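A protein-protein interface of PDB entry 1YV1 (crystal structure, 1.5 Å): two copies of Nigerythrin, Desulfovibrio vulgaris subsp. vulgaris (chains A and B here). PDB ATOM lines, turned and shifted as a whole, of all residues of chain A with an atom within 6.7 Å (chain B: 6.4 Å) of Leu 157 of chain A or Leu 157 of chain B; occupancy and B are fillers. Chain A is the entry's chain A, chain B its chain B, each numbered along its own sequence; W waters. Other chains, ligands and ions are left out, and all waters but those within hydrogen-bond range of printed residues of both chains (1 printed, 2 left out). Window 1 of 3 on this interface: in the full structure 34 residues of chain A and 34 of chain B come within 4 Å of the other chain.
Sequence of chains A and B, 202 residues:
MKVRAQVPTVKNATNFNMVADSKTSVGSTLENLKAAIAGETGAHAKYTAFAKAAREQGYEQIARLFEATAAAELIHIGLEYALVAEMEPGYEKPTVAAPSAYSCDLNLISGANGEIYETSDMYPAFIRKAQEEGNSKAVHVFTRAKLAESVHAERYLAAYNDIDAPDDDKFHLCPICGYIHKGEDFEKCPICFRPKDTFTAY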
ATOM      1  N   LEU A  65     -29.527 -18.722   4.041  1.00  0.00           N
ATOM      2  CA  LEU A  65     -29.086 -17.713   3.082  1.00  0.00           C
ATOM      3  C   LEU A  65     -27.573 -17.553   3.188  1.00  0.00           C
ATOM      4  O   LEU A  65     -26.882 -17.442   2.178  1.00  0.00           O
ATOM      5  CB  LEU A  65     -29.765 -16.369   3.351  1.00  0.00           C
ATOM      6  CG  LEU A  65     -29.303 -15.194   2.476  1.00  0.00           C
ATOM      7  CD1 LEU A  65     -29.510 -15.509   0.999  1.00  0.00           C
ATOM      8  CD2 LEU A  65     -30.085 -13.947   2.875  1.00  0.00           C
ATOM      9  N   LEU A 108     -25.683  -9.603   8.887  1.00  0.00           N
ATOM     10  CA  LEU A 108     -26.299  -9.357   7.586  1.00  0.00           C
ATOM     11  C   LEU A 108     -25.763  -8.048   7.009  1.00  0.00           C
ATOM     12  O   LEU A 108     -25.490  -7.950   5.810  1.00  0.00           O
ATOM     13  CB  LEU A 108     -27.822  -9.281   7.725  1.00  0.00           C
ATOM     14  CG  LEU A 108     -28.541 -10.624   7.869  1.00  0.00           C
ATOM     15  CD1 LEU A 108     -29.985 -10.416   8.313  1.00  0.00           C
ATOM     16  CD2 LEU A 108     -28.485 -11.370   6.537  1.00  0.00           C
ATOM     17  N   ILE A 109     -25.610  -7.045   7.868  1.00  0.00           N
ATOM     18  CA  ILE A 109     -25.093  -5.748   7.448  1.00  0.00           C
ATOM     19  C   ILE A 109     -23.627  -5.869   7.042  1.00  0.00           C
ATOM     20  O   ILE A 109     -23.215  -5.320   6.023  1.00  0.00           O
ATOM     21  CB  ILE A 109     -25.235  -4.701   8.580  1.00  0.00           C
ATOM     22  CG1 ILE A 109     -26.718  -4.402   8.829  1.00  0.00           C
ATOM     23  CG2 ILE A 109     -24.472  -3.426   8.223  1.00  0.00           C
ATOM     24  CD1 ILE A 109     -27.428  -3.688   7.672  1.00  0.00           C
ATOM     25  N   ALA A 112     -23.577  -7.384   3.679  1.00  0.00           N
ATOM     26  CA  ALA A 112     -23.982  -6.426   2.656  1.00  0.00           C
ATOM     27  C   ALA A 112     -22.862  -5.441   2.338  1.00  0.00           C
ATOM     28  O   ALA A 112     -22.610  -5.134   1.174  1.00  0.00           O
ATOM     29  CB  ALA A 112     -25.225  -5.673   3.112  1.00  0.00           C
ATOM     30  N   ASN A 113     -22.189  -4.946   3.372  1.00  0.00           N
ATOM     31  CA  ASN A 113     -21.110  -3.989   3.176  1.00  0.00           C
ATOM     32  C   ASN A 113     -19.972  -4.573   2.341  1.00  0.00           C
ATOM     33  O   ASN A 113     -19.419  -3.891   1.477  1.00  0.00           O
ATOM     34  CB  ASN A 113     -20.599  -3.497   4.537  1.00  0.00           C
ATOM     35  CG  ASN A 113     -21.565  -2.512   5.198  1.00  0.00           C
ATOM     36  OD1 ASN A 113     -21.500  -2.267   6.402  1.00  0.00           O
ATOM     37  ND2 ASN A 113     -22.460  -1.939   4.403  1.00  0.00           N
ATOM     38  N   ILE A 116     -21.124  -4.935  -1.311  1.00  0.00           N
ATOM     39  CA  ILE A 116     -21.153  -3.637  -1.968  1.00  0.00           C
ATOM     40  C   ILE A 116     -19.748  -3.195  -2.369  1.00  0.00           C
ATOM     41  O   ILE A 116     -19.548  -2.668  -3.462  1.00  0.00           O
ATOM     42  CB  ILE A 116     -21.822  -2.587  -1.056  1.00  0.00           C
ATOM     43  CG1 ILE A 116     -23.320  -2.898  -0.962  1.00  0.00           C
ATOM     44  CG2 ILE A 116     -21.587  -1.179  -1.599  1.00  0.00           C
ATOM     45  CD1 ILE A 116     -24.063  -2.102   0.087  1.00  0.00           C
ATOM     46  N   THR A 119     -18.745  -5.299  -5.468  1.00  0.00           N
ATOM     47  CA  THR A 119     -19.451  -4.997  -6.704  1.00  0.00           C
ATOM     48  C   THR A 119     -19.224  -3.594  -7.269  1.00  0.00           C
ATOM     49  O   THR A 119     -19.323  -3.396  -8.481  1.00  0.00           O
ATOM     50  CB  THR A 119     -20.980  -5.220  -6.543  1.00  0.00           C
ATOM     51  OG1 THR A 119     -21.562  -5.443  -7.833  1.00  0.00           O
ATOM     52  CG2 THR A 119     -21.647  -4.000  -5.894  1.00  0.00           C
ATOM     53  N   SER A 150     -23.655  -7.981  -6.121  1.00  0.00           N
ATOM     54  CA  SER A 150     -24.691  -6.977  -5.893  1.00  0.00           C
ATOM     55  C   SER A 150     -26.026  -7.656  -5.589  1.00  0.00           C
ATOM     56  O   SER A 150     -26.845  -7.115  -4.847  1.00  0.00           O
ATOM     57  CB  SER A 150     -24.805  -6.012  -7.081  1.00  0.00           C
ATOM     58  OG  SER A 150     -25.101  -6.674  -8.291  1.00  0.00           O
ATOM     59  N   HIS A 152     -26.226 -10.523  -3.966  1.00  0.00           N
ATOM     60  CA  HIS A 152     -26.048 -10.960  -2.582  1.00  0.00           C
ATOM     61  C   HIS A 152     -26.352  -9.811  -1.620  1.00  0.00           C
ATOM     62  O   HIS A 152     -26.991 -10.009  -0.586  1.00  0.00           O
ATOM     63  CB  HIS A 152     -24.634 -11.414  -2.338  1.00  0.00           C
ATOM     64  CG  HIS A 152     -24.238 -12.638  -3.158  1.00  0.00           C
ATOM     65  ND1 HIS A 152     -22.933 -13.063  -3.286  1.00  0.00           N
ATOM     66  CD2 HIS A 152     -24.989 -13.507  -3.873  1.00  0.00           C
ATOM     67  CE1 HIS A 152     -22.897 -14.141  -4.048  1.00  0.00           C
ATOM     68  NE2 HIS A 152     -24.131 -14.434  -4.416  1.00  0.00           N
ATOM     69  N   ALA A 153     -25.886  -8.614  -1.966  1.00  0.00           N
ATOM     70  CA  ALA A 153     -26.118  -7.440  -1.132  1.00  0.00           C
ATOM     71  C   ALA A 153     -27.608  -7.200  -0.945  1.00  0.00           C
ATOM     72  O   ALA A 153     -28.068  -6.969   0.171  1.00  0.00           O
ATOM     73  CB  ALA A 153     -25.471  -6.212  -1.761  1.00  0.00           C
ATOM     74  N   GLU A 154     -28.362  -7.253  -2.039  1.00  0.00           N
ATOM     75  CA  GLU A 154     -29.798  -7.034  -1.959  1.00  0.00           C
ATOM     76  C   GLU A 154     -30.468  -8.120  -1.119  1.00  0.00           C
ATOM     77  O   GLU A 154     -31.356  -7.830  -0.320  1.00  0.00           O
ATOM     78  CB  GLU A 154     -30.419  -6.995  -3.361  1.00  0.00           C
ATOM     79  CG  GLU A 154     -31.925  -6.753  -3.338  1.00  0.00           C
ATOM     80  CD  GLU A 154     -32.571  -6.781  -4.712  1.00  0.00           C
ATOM     81  OE1 GLU A 154     -33.816  -6.749  -4.767  1.00  0.00           O
ATOM     82  OE2 GLU A 154     -31.846  -6.830  -5.731  1.00  0.00           O
ATOM     83  N   ARG A 155     -30.039  -9.365  -1.289  1.00  0.00           N
ATOM     84  CA  ARG A 155     -30.620 -10.466  -0.525  1.00  0.00           C
ATOM     85  C   ARG A 155     -30.388 -10.268   0.971  1.00  0.00           C
ATOM     86  O   ARG A 155     -31.268 -10.545   1.790  1.00  0.00           O
ATOM     87  CB  ARG A 155     -30.015 -11.802  -0.969  1.00  0.00           C
ATOM     88  CG  ARG A 155     -30.475 -12.274  -2.346  1.00  0.00           C
ATOM     89  CD  ARG A 155     -31.632 -13.258  -2.239  1.00  0.00           C
ATOM     90  NE  ARG A 155     -32.755 -12.722  -1.478  1.00  0.00           N
ATOM     91  CZ  ARG A 155     -33.643 -11.858  -1.957  1.00  0.00           C
ATOM     92  NH1 ARG A 155     -33.543 -11.429  -3.207  1.00  0.00           N
ATOM     93  NH2 ARG A 155     -34.630 -11.423  -1.181  1.00  0.00           N
ATOM     94  N   TYR A 156     -29.204  -9.784   1.326  1.00  0.00           N
ATOM     95  CA  TYR A 156     -28.879  -9.550   2.727  1.00  0.00           C
ATOM     96  C   TYR A 156     -29.723  -8.416   3.313  1.00  0.00           C
ATOM     97  O   TYR A 156     -30.182  -8.505   4.456  1.00  0.00           O
ATOM     98  CB  TYR A 156     -27.383  -9.249   2.875  1.00  0.00           C
ATOM     99  CG  TYR A 156     -26.493 -10.484   2.819  1.00  0.00           C
ATOM    100  CD1 TYR A 156     -25.173 -10.395   2.379  1.00  0.00           C
ATOM    101  CD2 TYR A 156     -26.954 -11.727   3.258  1.00  0.00           C
ATOM    102  CE1 TYR A 156     -24.332 -11.510   2.379  1.00  0.00           C
ATOM    103  CE2 TYR A 156     -26.122 -12.849   3.266  1.00  0.00           C
ATOM    104  CZ  TYR A 156     -24.813 -12.733   2.828  1.00  0.00           C
ATOM    105  OH  TYR A 156     -23.981 -13.835   2.867  1.00  0.00           O
ATOM    106  N   LEU A 157     -29.941  -7.355   2.540  1.00  0.00           N
ATOM    107  CA  LEU A 157     -30.754  -6.249   3.037  1.00  0.00           C
ATOM    108  C   LEU A 157     -32.215  -6.665   3.155  1.00  0.00           C
ATOM    109  O   LEU A 157     -32.910  -6.237   4.071  1.00  0.00           O
ATOM    110  CB  LEU A 157     -30.630  -5.020   2.130  1.00  0.00           C
ATOM    111  CG  LEU A 157     -29.810  -3.841   2.673  1.00  0.00           C
ATOM    112  CD1 LEU A 157     -30.469  -3.291   3.936  1.00  0.00           C
ATOM    113  CD2 LEU A 157     -28.390  -4.280   2.958  1.00  0.00           C
ATOM    114  N   ALA A 158     -32.686  -7.503   2.237  1.00  0.00           N
ATOM    115  CA  ALA A 158     -34.069  -7.958   2.299  1.00  0.00           C
ATOM    116  C   ALA A 158     -34.267  -8.782   3.568  1.00  0.00           C
ATOM    117  O   ALA A 158     -35.272  -8.632   4.265  1.00  0.00           O
ATOM    118  CB  ALA A 158     -34.411  -8.786   1.072  1.00  0.00           C
ATOM    119  N   ALA A 159     -33.299  -9.646   3.866  1.00  0.00           N
ATOM    120  CA  ALA A 159     -33.361 -10.492   5.053  1.00  0.00           C
ATOM    121  C   ALA A 159     -33.305  -9.653   6.328  1.00  0.00           C
ATOM    122  O   ALA A 159     -33.957  -9.970   7.322  1.00  0.00           O
ATOM    123  CB  ALA A 159     -32.211 -11.501   5.038  1.00  0.00           C
ATOM    124  N   TYR A 160     -32.516  -8.583   6.292  1.00  0.00           N
ATOM    125  CA  TYR A 160     -32.378  -7.685   7.433  1.00  0.00           C
ATOM    126  C   TYR A 160     -33.719  -6.994   7.699  1.00  0.00           C
ATOM    127  O   TYR A 160     -34.166  -6.910   8.841  1.00  0.00           O
ATOM    128  CB  TYR A 160     -31.300  -6.643   7.127  1.00  0.00           C
ATOM    129  CG  TYR A 160     -31.041  -5.618   8.211  1.00  0.00           C
ATOM    130  CD1 TYR A 160     -30.112  -5.859   9.227  1.00  0.00           C
ATOM    131  CD2 TYR A 160     -31.676  -4.375   8.182  1.00  0.00           C
ATOM    132  CE1 TYR A 160     -29.813  -4.879  10.178  1.00  0.00           C
ATOM    133  CE2 TYR A 160     -31.388  -3.395   9.125  1.00  0.00           C
ATOM    134  CZ  TYR A 160     -30.453  -3.652  10.117  1.00  0.00           C
ATOM    135  OH  TYR A 160     -30.146  -2.669  11.032  1.00  0.00           O
ATOM    136  N   ASN A 161     -34.362  -6.504   6.644  1.00  0.00           N
ATOM    137  CA  ASN A 161     -35.642  -5.818   6.802  1.00  0.00           C
ATOM    138  C   ASN A 161     -36.754  -6.735   7.294  1.00  0.00           C
ATOM    139  O   ASN A 161     -37.694  -6.278   7.951  1.00  0.00           O
ATOM    140  CB  ASN A 161     -36.059  -5.147   5.489  1.00  0.00           C
ATOM    141  CG  ASN A 161     -35.182  -3.967   5.151  1.00  0.00           C
ATOM    142  OD1 ASN A 161     -34.680  -3.299   6.049  1.00  0.00           O
ATOM    143  ND2 ASN A 161     -35.001  -3.696   3.863  1.00  0.00           N
ATOM    144  N   ASP A 162     -36.643  -8.022   6.975  1.00  0.00           N
ATOM    145  CA  ASP A 162     -37.636  -9.012   7.388  1.00  0.00           C
ATOM    146  C   ASP A 162     -37.046 -10.002   8.389  1.00  0.00           C
ATOM    147  O   ASP A 162     -37.471 -11.150   8.453  1.00  0.00           O
ATOM    148  CB  ASP A 162     -38.158  -9.792   6.176  1.00  0.00           C
ATOM    149  CG  ASP A 162     -39.049  -8.958   5.286  1.00  0.00           C
ATOM    150  OD1 ASP A 162     -39.787  -8.110   5.827  1.00  0.00           O
ATOM    151  OD2 ASP A 162     -39.026  -9.164   4.052  1.00  0.00           O
ATOM    152  N   LEU B 108     -26.426   5.417  -6.652  1.00  0.00           N
ATOM    153  CA  LEU B 108     -27.250   4.435  -5.950  1.00  0.00           C
ATOM    154  C   LEU B 108     -26.438   3.766  -4.842  1.00  0.00           C
ATOM    155  O   LEU B 108     -26.951   3.515  -3.754  1.00  0.00           O
ATOM    156  CB  LEU B 108     -27.764   3.375  -6.925  1.00  0.00           C
ATOM    157  CG  LEU B 108     -28.877   3.858  -7.855  1.00  0.00           C
ATOM    158  CD1 LEU B 108     -29.135   2.826  -8.942  1.00  0.00           C
ATOM    159  CD2 LEU B 108     -30.131   4.106  -7.039  1.00  0.00           C
ATOM    160  N   ILE B 109     -25.170   3.471  -5.123  1.00  0.00           N
ATOM    161  CA  ILE B 109     -24.301   2.852  -4.128  1.00  0.00           C
ATOM    162  C   ILE B 109     -24.037   3.837  -2.986  1.00  0.00           C
ATOM    163  O   ILE B 109     -24.073   3.460  -1.816  1.00  0.00           O
ATOM    164  CB  ILE B 109     -22.955   2.403  -4.753  1.00  0.00           C
ATOM    165  CG1 ILE B 109     -23.197   1.267  -5.755  1.00  0.00           C
ATOM    166  CG2 ILE B 109     -21.996   1.953  -3.658  1.00  0.00           C
ATOM    167  CD1 ILE B 109     -23.737  -0.020  -5.134  1.00  0.00           C
ATOM    168  N   ALA B 112     -27.117   3.835  -0.908  1.00  0.00           N
ATOM    169  CA  ALA B 112     -27.217   2.618  -0.112  1.00  0.00           C
ATOM    170  C   ALA B 112     -26.264   2.640   1.079  1.00  0.00           C
ATOM    171  O   ALA B 112     -26.648   2.267   2.186  1.00  0.00           O
ATOM    172  CB  ALA B 112     -26.932   1.402  -0.978  1.00  0.00           C
ATOM    173  N   ILE B 116     -27.363   2.436   4.963  1.00  0.00           N
ATOM    174  CA  ILE B 116     -26.882   1.355   5.815  1.00  0.00           C
ATOM    175  C   ILE B 116     -26.217   1.909   7.072  1.00  0.00           C
ATOM    176  O   ILE B 116     -26.428   1.397   8.173  1.00  0.00           O
ATOM    177  CB  ILE B 116     -25.905   0.448   5.034  1.00  0.00           C
ATOM    178  CG1 ILE B 116     -26.696  -0.348   3.990  1.00  0.00           C
ATOM    179  CG2 ILE B 116     -25.164  -0.480   5.986  1.00  0.00           C
ATOM    180  CD1 ILE B 116     -25.840  -1.093   2.991  1.00  0.00           C
ATOM    181  N   THR B 119     -29.086   3.138   9.412  1.00  0.00           N
ATOM    182  CA  THR B 119     -29.912   2.097  10.000  1.00  0.00           C
ATOM    183  C   THR B 119     -29.186   1.131  10.929  1.00  0.00           C
ATOM    184  O   THR B 119     -29.800   0.581  11.841  1.00  0.00           O
ATOM    185  CB  THR B 119     -30.642   1.285   8.898  1.00  0.00           C
ATOM    186  OG1 THR B 119     -31.828   0.697   9.447  1.00  0.00           O
ATOM    187  CG2 THR B 119     -29.744   0.176   8.346  1.00  0.00           C
ATOM    188  N   GLU B 149     -34.906   3.800   6.730  1.00  0.00           N
ATOM    189  CA  GLU B 149     -33.603   3.819   6.068  1.00  0.00           C
ATOM    190  C   GLU B 149     -33.179   2.456   5.543  1.00  0.00           C
ATOM    191  O   GLU B 149     -32.605   2.371   4.461  1.00  0.00           O
ATOM    192  CB  GLU B 149     -32.511   4.351   7.005  1.00  0.00           C
ATOM    193  CG  GLU B 149     -32.907   5.551   7.853  1.00  0.00           C
ATOM    194  CD  GLU B 149     -33.297   6.792   7.069  1.00  0.00           C
ATOM    195  OE1 GLU B 149     -33.644   6.661   5.886  1.00  0.00           O
ATOM    196  OE2 GLU B 149     -33.259   7.898   7.657  1.00  0.00           O
ATOM    197  N   SER B 150     -33.440   1.385   6.290  1.00  0.00           N
ATOM    198  CA  SER B 150     -33.031   0.078   5.793  1.00  0.00           C
ATOM    199  C   SER B 150     -33.869  -0.299   4.574  1.00  0.00           C
ATOM    200  O   SER B 150     -33.399  -1.015   3.684  1.00  0.00           O
ATOM    201  CB  SER B 150     -33.122  -0.981   6.894  1.00  0.00           C
ATOM    202  OG  SER B 150     -34.423  -1.083   7.429  1.00  0.00           O
ATOM    203  N   VAL B 151     -35.105   0.191   4.525  1.00  0.00           N
ATOM    204  CA  VAL B 151     -35.963  -0.067   3.373  1.00  0.00           C
ATOM    205  C   VAL B 151     -35.380   0.708   2.190  1.00  0.00           C
ATOM    206  O   VAL B 151     -35.332   0.206   1.065  1.00  0.00           O
ATOM    207  CB  VAL B 151     -37.418   0.383   3.647  1.00  0.00           C
ATOM    208  CG1 VAL B 151     -38.195   0.493   2.344  1.00  0.00           C
ATOM    209  CG2 VAL B 151     -38.092  -0.621   4.571  1.00  0.00           C
ATOM    210  N   HIS B 152     -34.924   1.931   2.442  1.00  0.00           N
ATOM    211  CA  HIS B 152     -34.320   2.736   1.376  1.00  0.00           C
ATOM    212  C   HIS B 152     -33.113   2.047   0.827  1.00  0.00           C
ATOM    213  O   HIS B 152     -32.900   2.011  -0.382  1.00  0.00           O
ATOM    214  CB  HIS B 152     -33.908   4.101   1.929  1.00  0.00           C
ATOM    215  CG  HIS B 152     -35.075   4.957   2.416  1.00  0.00           C
ATOM    216  ND1 HIS B 152     -34.898   6.105   3.158  1.00  0.00           N
ATOM    217  CD2 HIS B 152     -36.413   4.819   2.250  1.00  0.00           C
ATOM    218  CE1 HIS B 152     -36.076   6.636   3.431  1.00  0.00           C
ATOM    219  NE2 HIS B 152     -37.013   5.876   2.891  1.00  0.00           N
ATOM    220  N   ALA B 153     -32.316   1.470   1.718  1.00  0.00           N
ATOM    221  CA  ALA B 153     -31.114   0.760   1.306  1.00  0.00           C
ATOM    222  C   ALA B 153     -31.467  -0.354   0.332  1.00  0.00           C
ATOM    223  O   ALA B 153     -30.847  -0.488  -0.722  1.00  0.00           O
ATOM    224  CB  ALA B 153     -30.412   0.176   2.524  1.00  0.00           C
ATOM    225  N   GLU B 154     -32.468  -1.154   0.684  1.00  0.00           N
ATOM    226  CA  GLU B 154     -32.871  -2.258  -0.177  1.00  0.00           C
ATOM    227  C   GLU B 154     -33.387  -1.767  -1.527  1.00  0.00           C
ATOM    228  O   GLU B 154     -33.073  -2.349  -2.567  1.00  0.00           O
ATOM    229  CB  GLU B 154     -33.942  -3.117   0.510  1.00  0.00           C
ATOM    230  CG  GLU B 154     -34.379  -4.305  -0.339  1.00  0.00           C
ATOM    231  CD  GLU B 154     -35.457  -5.157   0.305  1.00  0.00           C
ATOM    232  OE1 GLU B 154     -35.936  -6.095  -0.367  1.00  0.00           O
ATOM    233  OE2 GLU B 154     -35.829  -4.901   1.472  1.00  0.00           O
ATOM    234  N   ARG B 155     -34.171  -0.693  -1.516  1.00  0.00           N
ATOM    235  CA  ARG B 155     -34.710  -0.152  -2.757  1.00  0.00           C
ATOM    236  C   ARG B 155     -33.583   0.310  -3.673  1.00  0.00           C
ATOM    237  O   ARG B 155     -33.641   0.119  -4.885  1.00  0.00           O
ATOM    238  CB  ARG B 155     -35.660   1.014  -2.457  1.00  0.00           C
ATOM    239  CG  ARG B 155     -36.973   0.584  -1.802  1.00  0.00           C
ATOM    240  CD  ARG B 155     -38.087   0.419  -2.828  1.00  0.00           C
ATOM    241  NE  ARG B 155     -37.736  -0.475  -3.927  1.00  0.00           N
ATOM    242  CZ  ARG B 155     -37.702  -1.802  -3.838  1.00  0.00           C
ATOM    243  NH1 ARG B 155     -37.996  -2.399  -2.692  1.00  0.00           N
ATOM    244  NH2 ARG B 155     -37.386  -2.532  -4.905  1.00  0.00           N
ATOM    245  N   TYR B 156     -32.551   0.908  -3.091  1.00  0.00           N
ATOM    246  CA  TYR B 156     -31.420   1.385  -3.879  1.00  0.00           C
ATOM    247  C   TYR B 156     -30.639   0.225  -4.485  1.00  0.00           C
ATOM    248  O   TYR B 156     -30.228   0.281  -5.643  1.00  0.00           O
ATOM    249  CB  TYR B 156     -30.497   2.256  -3.014  1.00  0.00           C
ATOM    250  CG  TYR B 156     -30.999   3.672  -2.787  1.00  0.00           C
ATOM    251  CD1 TYR B 156     -30.648   4.376  -1.637  1.00  0.00           C
ATOM    252  CD2 TYR B 156     -31.787   4.322  -3.740  1.00  0.00           C
ATOM    253  CE1 TYR B 156     -31.064   5.694  -1.441  1.00  0.00           C
ATOM    254  CE2 TYR B 156     -32.207   5.638  -3.554  1.00  0.00           C
ATOM    255  CZ  TYR B 156     -31.840   6.317  -2.405  1.00  0.00           C
ATOM    256  OH  TYR B 156     -32.241   7.622  -2.221  1.00  0.00           O
ATOM    257  N   LEU B 157     -30.438  -0.834  -3.709  1.00  0.00           N
ATOM    258  CA  LEU B 157     -29.698  -1.981  -4.218  1.00  0.00           C
ATOM    259  C   LEU B 157     -30.495  -2.672  -5.320  1.00  0.00           C
ATOM    260  O   LEU B 157     -29.924  -3.134  -6.306  1.00  0.00           O
ATOM    261  CB  LEU B 157     -29.378  -2.953  -3.075  1.00  0.00           C
ATOM    262  CG  LEU B 157     -28.472  -2.365  -1.984  1.00  0.00           C
ATOM    263  CD1 LEU B 157     -28.401  -3.310  -0.806  1.00  0.00           C
ATOM    264  CD2 LEU B 157     -27.084  -2.099  -2.548  1.00  0.00           C
ATOM    265  N   ALA B 158     -31.813  -2.736  -5.157  1.00  0.00           N
ATOM    266  CA  ALA B 158     -32.669  -3.352  -6.161  1.00  0.00           C
ATOM    267  C   ALA B 158     -32.585  -2.566  -7.472  1.00  0.00           C
ATOM    268  O   ALA B 158     -32.486  -3.149  -8.552  1.00  0.00           O
ATOM    269  CB  ALA B 158     -34.114  -3.390  -5.665  1.00  0.00           C
ATOM    270  N   ALA B 159     -32.621  -1.241  -7.375  1.00  0.00           N
ATOM    271  CA  ALA B 159     -32.549  -0.402  -8.564  1.00  0.00           C
ATOM    272  C   ALA B 159     -31.191  -0.532  -9.245  1.00  0.00           C
ATOM    273  O   ALA B 159     -31.094  -0.459 -10.465  1.00  0.00           O
ATOM    274  CB  ALA B 159     -32.814   1.046  -8.195  1.00  0.00           C
ATOM    275  N   TYR B 160     -30.145  -0.719  -8.446  1.00  0.00           N
ATOM    276  CA  TYR B 160     -28.785  -0.878  -8.957  1.00  0.00           C
ATOM    277  C   TYR B 160     -28.692  -2.174  -9.765  1.00  0.00           C
ATOM    278  O   TYR B 160     -28.159  -2.196 -10.877  1.00  0.00           O
ATOM    279  CB  TYR B 160     -27.808  -0.929  -7.781  1.00  0.00           C
ATOM    280  CG  TYR B 160     -26.349  -1.100  -8.149  1.00  0.00           C
ATOM    281  CD1 TYR B 160     -25.550  -0.001  -8.466  1.00  0.00           C
ATOM    282  CD2 TYR B 160     -25.752  -2.360  -8.122  1.00  0.00           C
ATOM    283  CE1 TYR B 160     -24.186  -0.156  -8.739  1.00  0.00           C
ATOM    284  CE2 TYR B 160     -24.398  -2.524  -8.393  1.00  0.00           C
ATOM    285  CZ  TYR B 160     -23.618  -1.422  -8.699  1.00  0.00           C
ATOM    286  OH  TYR B 160     -22.272  -1.588  -8.958  1.00  0.00           O
ATOM    287  N   ASN B 161     -29.221  -3.256  -9.202  1.00  0.00           N
ATOM    288  CA  ASN B 161     -29.187  -4.550  -9.876  1.00  0.00           C
ATOM    289  C   ASN B 161     -29.986  -4.558 -11.164  1.00  0.00           C
ATOM    290  O   ASN B 161     -29.648  -5.281 -12.097  1.00  0.00           O
ATOM    291  CB  ASN B 161     -29.699  -5.649  -8.944  1.00  0.00           C
ATOM    292  CG  ASN B 161     -28.735  -5.937  -7.825  1.00  0.00           C
ATOM    293  OD1 ASN B 161     -27.533  -5.751  -7.988  1.00  0.00           O
ATOM    294  ND2 ASN B 161     -29.242  -6.403  -6.693  1.00  0.00           N
ATOM    295  N   ASP B 162     -31.046  -3.753 -11.207  1.00  0.00           N
ATOM    296  CA  ASP B 162     -31.902  -3.657 -12.389  1.00  0.00           C
ATOM    297  C   ASP B 162     -31.738  -2.307 -13.081  1.00  0.00           C
ATOM    298  O   ASP B 162     -32.666  -1.814 -13.719  1.00  0.00           O
ATOM    299  CB  ASP B 162     -33.376  -3.833 -11.999  1.00  0.00           C
ATOM    300  CG  ASP B 162     -33.684  -5.221 -11.495  1.00  0.00           C
ATOM    301  OD1 ASP B 162     -33.104  -6.186 -12.035  1.00  0.00           O
ATOM    302  OD2 ASP B 162     -34.520  -5.350 -10.572  1.00  0.00           O
HETATM  303  O   HOH W   1     -35.810  -6.542  -3.010  1.00  0.00           O
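The side-chain hydroxyl (OH) of Tyr 160 of chain B sits at hydrogen-bond distance from the backbone carbonyl oxygen (O) of Thr 119 of chain A, 3.5 Å away.
The side-chain amide oxygen (OD1) of Asn 161 of chain B is in hydrogen-bond range of the side-chain hydroxyl (OG) of Ser 150 of chain A.
The side-chain carboxylate (OE2) of Glu 154 of chain A sits at hydrogen-bond distance from the side-chain amide nitrogen (ND2) of Asn 161 of chain B, at 2.8 Å.
OH of Tyr 160 of chain A is in hydrogen-bond range of O of Thr 119 of chain B.
OD1 of Asn 161 of chain A sits at hydrogen-bond distance from OG of Ser 150 of chain B, 2.6 Å away.
ND2 of Asn 161 of chain A lies within hydrogen-bond range of OE2 of Glu 154 of chain B, 2.8 Å away.
O of Leu 157 of chain B lies within hydrogen-bond range of ND2 of Asn 161 of chain B, 3.4 Å away.
Among the printed residues, merely in contact across the chains: Ile 109 of chain A with Ile 116 of chain B (3.8 Å), Asn 113 of chain A with Ile 116 of chain B (3.5 Å), Ile 116 of chain A with Ile 109 of chain B (3.8 Å), Ile 116 of chain A with Ile 116 of chain B (3.6 Å), Ser 150 of chain A with Tyr 160 of chain B (3.7 Å), Ala 153 of chain A with Leu 157 of chain B (3.8 Å), Glu 154 of chain A with Ala 158 of chain B (3.5 Å), Leu 157 of chain A with Ser 150 of chain B (3.7 Å), Leu 157 of chain A with Ala 153 of chain B (3.7 Å), Leu 157 of chain A with Leu 157 of chain B (3.8 Å), Ala 158 of chain A with Glu 154 of chain B (3.4 Å), Tyr 160 of chain A with Ser 150 of chain B (3.7 Å) and Asn 161 of chain A with Val 151 of chain B (3.8 Å).
Leu 157 of chain A touches just these residues of chain B: Ser 150 (3.7 Å), Ala 153 (3.7 Å) and Leu 157 (3.8 Å).
Of the printed residues of chain A, Val 151 of chain B touches Asn 161 (3.8 Å).
Printed residues of chain A within 4 Å of Ala 158 of chain B: Glu 154.
His 152 of chain B touches none of the printed residues of chain A.
The nearest printed residue of chain A that does not touch Leu 157 of chain B is Ile 116 of chain A (4.01 Å).
The nearest printed residue of chain A that does not touch Glu 154 of chain B is Leu 157 of chain A (4.1 Å).
Of the 19 printed residues of chain A, 11 touch a printed residue of chain B.
Hydrophobic or aromatic side chains of chain A that line the printed part of chain B: Ile 109, Ile 116, Leu 157, Ala 158 and Tyr 160.
Of the 19 printed residues of chain B, 11 touch a printed residue of chain A.
Among the printed residues, 19 pairs touch across the chains.
Among the printed residues, no Asp or Glu carboxylate lies within 4 Å of a Lys or Arg side-chain nitrogen of the other chain.
Ala 153 of chain A touches Leu 157 of chain B, and with the chains exchanged Leu 157 of chain A touches Ala 153 of chain B.
Of the 19 pairs that touch across the chains among the printed residues, 16 have their exchanged pair printed and touching as well.
Water W1 lies within hydrogen-bond range of OE1 of Glu 154 of chain A and OE1 of Glu 154 of chain B.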
